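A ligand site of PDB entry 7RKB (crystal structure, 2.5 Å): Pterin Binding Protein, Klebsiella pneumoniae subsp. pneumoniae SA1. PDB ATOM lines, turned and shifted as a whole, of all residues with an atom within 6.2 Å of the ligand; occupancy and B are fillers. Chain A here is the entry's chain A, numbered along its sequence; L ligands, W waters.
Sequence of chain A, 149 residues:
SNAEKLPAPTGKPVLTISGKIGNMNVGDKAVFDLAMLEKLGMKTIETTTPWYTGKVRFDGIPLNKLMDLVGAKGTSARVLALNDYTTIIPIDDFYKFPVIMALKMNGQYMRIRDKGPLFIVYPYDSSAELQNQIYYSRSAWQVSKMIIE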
ATOM      1  N   PRO A  50       9.146 -10.758  -3.035  1.00  0.00           N
ATOM      2  CA  PRO A  50       9.167 -10.518  -4.475  1.00  0.00           C
ATOM      3  C   PRO A  50      10.092  -9.376  -4.889  1.00  0.00           C
ATOM      4  O   PRO A  50      10.183  -9.059  -6.075  1.00  0.00           O
ATOM      5  CB  PRO A  50       7.699 -10.161  -4.781  1.00  0.00           C
ATOM      6  CG  PRO A  50       7.188  -9.541  -3.505  1.00  0.00           C
ATOM      7  CD  PRO A  50       7.931 -10.247  -2.387  1.00  0.00           C
ATOM      8  N   TRP A  51      10.817  -8.794  -3.920  1.00  0.00           N
ATOM      9  CA  TRP A  51      11.696  -7.673  -4.191  1.00  0.00           C
ATOM     10  C   TRP A  51      13.167  -8.074  -4.131  1.00  0.00           C
ATOM     11  O   TRP A  51      14.011  -7.410  -4.726  1.00  0.00           O
ATOM     12  CB  TRP A  51      11.393  -6.566  -3.178  1.00  0.00           C
ATOM     13  CG  TRP A  51       9.933  -6.254  -3.144  1.00  0.00           C
ATOM     14  CD1 TRP A  51       9.162  -5.766  -4.159  1.00  0.00           C
ATOM     15  CD2 TRP A  51       9.035  -6.518  -2.053  1.00  0.00           C
ATOM     16  NE1 TRP A  51       7.859  -5.662  -3.753  1.00  0.00           N
ATOM     17  CE2 TRP A  51       7.750  -6.120  -2.471  1.00  0.00           C
ATOM     18  CE3 TRP A  51       9.197  -7.019  -0.760  1.00  0.00           C
ATOM     19  CZ2 TRP A  51       6.636  -6.221  -1.634  1.00  0.00           C
ATOM     20  CZ3 TRP A  51       8.098  -7.123   0.071  1.00  0.00           C
ATOM     21  CH2 TRP A  51       6.834  -6.727  -0.373  1.00  0.00           C
ATOM     22  N   ALA A  81       3.708   6.745   2.023  1.00  0.00           N
ATOM     23  CA  ALA A  81       5.158   6.660   1.868  1.00  0.00           C
ATOM     24  C   ALA A  81       5.721   8.069   1.866  1.00  0.00           C
ATOM     25  O   ALA A  81       4.996   9.043   1.711  1.00  0.00           O
ATOM     26  CB  ALA A  81       5.521   5.903   0.616  1.00  0.00           C
ATOM     27  N   LEU A  82       7.052   8.158   1.983  1.00  0.00           N
ATOM     28  CA  LEU A  82       7.745   9.425   2.081  1.00  0.00           C
ATOM     29  C   LEU A  82       7.383  10.337   0.901  1.00  0.00           C
ATOM     30  O   LEU A  82       7.337  11.552   1.062  1.00  0.00           O
ATOM     31  CB  LEU A  82       9.243   9.140   2.170  1.00  0.00           C
ATOM     32  CG  LEU A  82      10.126  10.335   2.537  1.00  0.00           C
ATOM     33  CD1 LEU A  82       9.973  10.649   4.026  1.00  0.00           C
ATOM     34  CD2 LEU A  82      11.579  10.059   2.184  1.00  0.00           C
ATOM     35  N   TYR A  85       3.365   7.121  -2.508  1.00  0.00           N
ATOM     36  CA  TYR A  85       2.707   5.829  -2.434  1.00  0.00           C
ATOM     37  C   TYR A  85       1.695   5.831  -1.294  1.00  0.00           C
ATOM     38  O   TYR A  85       1.924   6.455  -0.256  1.00  0.00           O
ATOM     39  CB  TYR A  85       3.692   4.667  -2.232  1.00  0.00           C
ATOM     40  CG  TYR A  85       3.041   3.311  -2.312  1.00  0.00           C
ATOM     41  CD1 TYR A  85       2.471   2.869  -3.498  1.00  0.00           C
ATOM     42  CD2 TYR A  85       2.930   2.496  -1.209  1.00  0.00           C
ATOM     43  CE1 TYR A  85       1.853   1.638  -3.599  1.00  0.00           C
ATOM     44  CE2 TYR A  85       2.310   1.256  -1.280  1.00  0.00           C
ATOM     45  CZ  TYR A  85       1.762   0.825  -2.482  1.00  0.00           C
ATOM     46  OH  TYR A  85       1.148  -0.402  -2.562  1.00  0.00           O
ATOM     47  N   PHE A 119       9.716   0.121   6.912  1.00  0.00           N
ATOM     48  CA  PHE A 119       9.164  -0.770   5.918  1.00  0.00           C
ATOM     49  C   PHE A 119       8.259  -1.809   6.575  1.00  0.00           C
ATOM     50  O   PHE A 119       8.692  -2.550   7.455  1.00  0.00           O
ATOM     51  CB  PHE A 119      10.323  -1.330   5.081  1.00  0.00           C
ATOM     52  CG  PHE A 119      10.012  -2.488   4.170  1.00  0.00           C
ATOM     53  CD1 PHE A 119       8.874  -2.487   3.370  1.00  0.00           C
ATOM     54  CD2 PHE A 119      10.962  -3.477   3.946  1.00  0.00           C
ATOM     55  CE1 PHE A 119       8.628  -3.538   2.507  1.00  0.00           C
ATOM     56  CE2 PHE A 119      10.726  -4.515   3.054  1.00  0.00           C
ATOM     57  CZ  PHE A 119       9.553  -4.548   2.338  1.00  0.00           C
ATOM     58  N   GLN A 133      -0.576 -10.302  -4.086  1.00  0.00           N
ATOM     59  CA  GLN A 133      -0.379  -8.875  -4.286  1.00  0.00           C
ATOM     60  C   GLN A 133      -1.060  -8.042  -3.190  1.00  0.00           C
ATOM     61  O   GLN A 133      -0.583  -6.945  -2.898  1.00  0.00           O
ATOM     62  CB  GLN A 133      -0.881  -8.471  -5.681  1.00  0.00           C
ATOM     63  CG  GLN A 133      -0.504  -7.049  -6.054  1.00  0.00           C
ATOM     64  CD  GLN A 133       0.998  -6.875  -6.020  1.00  0.00           C
ATOM     65  OE1 GLN A 133       1.736  -7.604  -6.680  1.00  0.00           O
ATOM     66  NE2 GLN A 133       1.470  -5.948  -5.197  1.00  0.00           N
ATOM     67  N   TYR A 136       1.457  -7.771  -0.657  1.00  0.00           N
ATOM     68  CA  TYR A 136       2.656  -7.122  -1.169  1.00  0.00           C
ATOM     69  C   TYR A 136       2.384  -5.623  -1.292  1.00  0.00           C
ATOM     70  O   TYR A 136       3.256  -4.820  -0.974  1.00  0.00           O
ATOM     71  CB  TYR A 136       3.103  -7.672  -2.521  1.00  0.00           C
ATOM     72  CG  TYR A 136       3.299  -9.172  -2.579  1.00  0.00           C
ATOM     73  CD1 TYR A 136       4.023  -9.850  -1.609  1.00  0.00           C
ATOM     74  CD2 TYR A 136       2.892  -9.884  -3.701  1.00  0.00           C
ATOM     75  CE1 TYR A 136       4.219 -11.211  -1.696  1.00  0.00           C
ATOM     76  CE2 TYR A 136       3.098 -11.253  -3.807  1.00  0.00           C
ATOM     77  CZ  TYR A 136       3.765 -11.914  -2.799  1.00  0.00           C
ATOM     78  OH  TYR A 136       3.958 -13.266  -2.897  1.00  0.00           O
ATOM     79  N   SER A 137       1.182  -5.261  -1.752  1.00  0.00           N
ATOM     80  CA  SER A 137       0.819  -3.862  -1.940  1.00  0.00           C
ATOM     81  C   SER A 137       0.735  -3.111  -0.613  1.00  0.00           C
ATOM     82  O   SER A 137       0.944  -1.905  -0.567  1.00  0.00           O
ATOM     83  CB  SER A 137      -0.481  -3.720  -2.703  1.00  0.00           C
ATOM     84  OG  SER A 137      -0.369  -4.261  -4.010  1.00  0.00           O
ATOM     85  N   ARG A 138       0.419  -3.844   0.463  1.00  0.00           N
ATOM     86  CA  ARG A 138       0.298  -3.259   1.788  1.00  0.00           C
ATOM     87  C   ARG A 138       1.660  -3.170   2.477  1.00  0.00           C
ATOM     88  O   ARG A 138       1.769  -2.581   3.549  1.00  0.00           O
ATOM     89  CB  ARG A 138      -0.687  -4.062   2.635  1.00  0.00           C
ATOM     90  CG  ARG A 138      -2.104  -3.998   2.110  1.00  0.00           C
ATOM     91  CD  ARG A 138      -3.043  -4.899   2.884  1.00  0.00           C
ATOM     92  NE  ARG A 138      -4.391  -4.842   2.345  1.00  0.00           N
ATOM     93  CZ  ARG A 138      -5.383  -5.622   2.759  1.00  0.00           C
ATOM     94  NH1 ARG A 138      -5.140  -6.563   3.654  1.00  0.00           N
ATOM     95  NH2 ARG A 138      -6.598  -5.478   2.241  1.00  0.00           N
ATOM     96  N   SER A 139       2.685  -3.773   1.855  1.00  0.00           N
ATOM     97  CA  SER A 139       4.030  -3.737   2.406  1.00  0.00           C
ATOM     98  C   SER A 139       4.713  -2.459   1.917  1.00  0.00           C
ATOM     99  O   SER A 139       5.641  -2.494   1.106  1.00  0.00           O
ATOM    100  CB  SER A 139       4.780  -4.978   2.029  1.00  0.00           C
ATOM    101  OG  SER A 139       4.114  -6.137   2.534  1.00  0.00           O
ATOM    102  N   ALA A 140       4.220  -1.324   2.424  1.00  0.00           N
ATOM    103  CA  ALA A 140       4.728  -0.023   2.038  1.00  0.00           C
ATOM    104  C   ALA A 140       6.105   0.220   2.651  1.00  0.00           C
ATOM    105  O   ALA A 140       6.322  -0.046   3.838  1.00  0.00           O
ATOM    106  CB  ALA A 140       3.757   1.061   2.444  1.00  0.00           C
ATOM    107  N   TRP A 141       7.015   0.740   1.823  1.00  0.00           N
ATOM    108  CA  TRP A 141       8.366   1.059   2.236  1.00  0.00           C
ATOM    109  C   TRP A 141       8.521   2.587   2.284  1.00  0.00           C
ATOM    110  O   TRP A 141       7.670   3.319   1.789  1.00  0.00           O
ATOM    111  CB  TRP A 141       9.389   0.336   1.345  1.00  0.00           C
ATOM    112  CG  TRP A 141       9.299   0.609  -0.131  1.00  0.00           C
ATOM    113  CD1 TRP A 141       9.535   1.788  -0.777  1.00  0.00           C
ATOM    114  CD2 TRP A 141       8.941  -0.344  -1.153  1.00  0.00           C
ATOM    115  NE1 TRP A 141       9.357   1.629  -2.125  1.00  0.00           N
ATOM    116  CE2 TRP A 141       8.990   0.332  -2.384  1.00  0.00           C
ATOM    117  CE3 TRP A 141       8.569  -1.692  -1.146  1.00  0.00           C
ATOM    118  CZ2 TRP A 141       8.696  -0.296  -3.592  1.00  0.00           C
ATOM    119  CZ3 TRP A 141       8.278  -2.316  -2.333  1.00  0.00           C
ATOM    120  CH2 TRP A 141       8.342  -1.629  -3.550  1.00  0.00           C
ATOM    121  N   GLN A 142       9.604   3.051   2.904  1.00  0.00           N
ATOM    122  CA  GLN A 142       9.847   4.482   3.053  1.00  0.00           C
ATOM    123  C   GLN A 142       8.607   5.107   3.697  1.00  0.00           C
ATOM    124  O   GLN A 142       8.139   6.159   3.275  1.00  0.00           O
ATOM    125  CB  GLN A 142      10.189   5.125   1.715  1.00  0.00           C
ATOM    126  CG  GLN A 142      11.446   4.547   1.076  1.00  0.00           C
ATOM    127  CD  GLN A 142      11.808   5.206  -0.237  1.00  0.00           C
ATOM    128  OE1 GLN A 142      11.127   6.118  -0.711  1.00  0.00           O
ATOM    129  NE2 GLN A 142      12.898   4.754  -0.831  1.00  0.00           N
ATOM    130  N   VAL A 143       8.089   4.419   4.727  1.00  0.00           N
ATOM    131  CA  VAL A 143       6.899   4.848   5.441  1.00  0.00           C
ATOM    132  C   VAL A 143       7.235   6.093   6.267  1.00  0.00           C
ATOM    133  O   VAL A 143       8.296   6.172   6.865  1.00  0.00           O
ATOM    134  CB  VAL A 143       6.397   3.716   6.355  1.00  0.00           C
ATOM    135  CG1 VAL A 143       5.213   4.142   7.204  1.00  0.00           C
ATOM    136  CG2 VAL A 143       6.082   2.464   5.564  1.00  0.00           C
HETATM  137  N1  LIG L   1       6.117   2.459  -2.859  1.00  0.00           N
HETATM  138  C1  LIG L   1       5.586   1.526  -3.726  1.00  0.00           C
HETATM  139  C2  LIG L   1       5.262   0.219  -3.174  1.00  0.00           C
HETATM  140  N2  LIG L   1       4.731  -0.763  -3.959  1.00  0.00           N
HETATM  141  C3  LIG L   1       4.452  -1.920  -3.394  1.00  0.00           C
HETATM  142  C4  LIG L   1       4.701  -2.140  -2.015  1.00  0.00           C
HETATM  143  N3  LIG L   1       5.215  -1.205  -1.234  1.00  0.00           N
HETATM  144  C5  LIG L   1       5.500   0.002  -1.807  1.00  0.00           C
HETATM  145  N4  LIG L   1       6.029   0.998  -1.001  1.00  0.00           N
HETATM  146  C6  LIG L   1       6.321   2.179  -1.532  1.00  0.00           C
HETATM  147  N5  LIG L   1       6.839   3.151  -0.770  1.00  0.00           N
HETATM  148  C7  LIG L   1       3.860  -3.030  -4.237  1.00  0.00           C
HETATM  149  O1  LIG L   1       4.729  -4.161  -4.246  1.00  0.00           O
HETATM  150  C8  LIG L   1       3.576  -2.603  -5.683  1.00  0.00           C
HETATM  151  O2  LIG L   1       4.778  -2.067  -6.247  1.00  0.00           O
HETATM  152  C9  LIG L   1       2.458  -1.590  -5.837  1.00  0.00           C
HETATM  153  O3  LIG L   1       1.253  -2.014  -5.211  1.00  0.00           O
HETATM  154  O4  LIG L   1       5.413   1.833  -4.902  1.00  0.00           O
HETATM  155  O   HOH W   1       4.664   4.837  -6.388  1.00  0.00           O
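The side-chain hydroxyl of Tyr 85 sits at hydrogen-bond distance from the backbone carbonyl oxygen of Ser 137. The side-chain amide nitrogen of Gln 133 lies within hydrogen-bond range of the side-chain hydroxyl of Ser 137 (2.8 Å).
Trp 51 touches the ligand. Ala 81 touches the ligand (CB to N5, 3.4 Å). Gln 133 touches the ligand. O of Tyr 136 touches C4 of the ligand, 3.2 Å away. CA of Ala 140 touches N4 of the ligand, at 3.5 Å. Hydrophobic or aromatic side chains that line the ligand: Trp 51, Ala 81, Tyr 85 and Trp 141. The nearest printed residue that does not touch the ligand is Gln 142 (4.6 Å).
N of Trp 141 sits at hydrogen-bond distance from N4 of the ligand, 3.0 Å away. A nitrogen (N5) of the ligand sits at hydrogen-bond distance from the backbone carbonyl oxygen of Trp 141, at 2.7 Å. A nitrogen (N1) of the ligand lies close to the indole nitrogen (NE1) of Trp 141, 3.4 Å away. O of Ser 139 lies close to N3 of the ligand, 2.7 Å away. OG of Ser 137 sits at hydrogen-bond distance from O3 of the ligand (3.0 Å). The side-chain hydroxyl (OH) of Tyr 85 lies within hydrogen-bond range of an oxygen (O3) of the ligand, at 3.1 Å.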
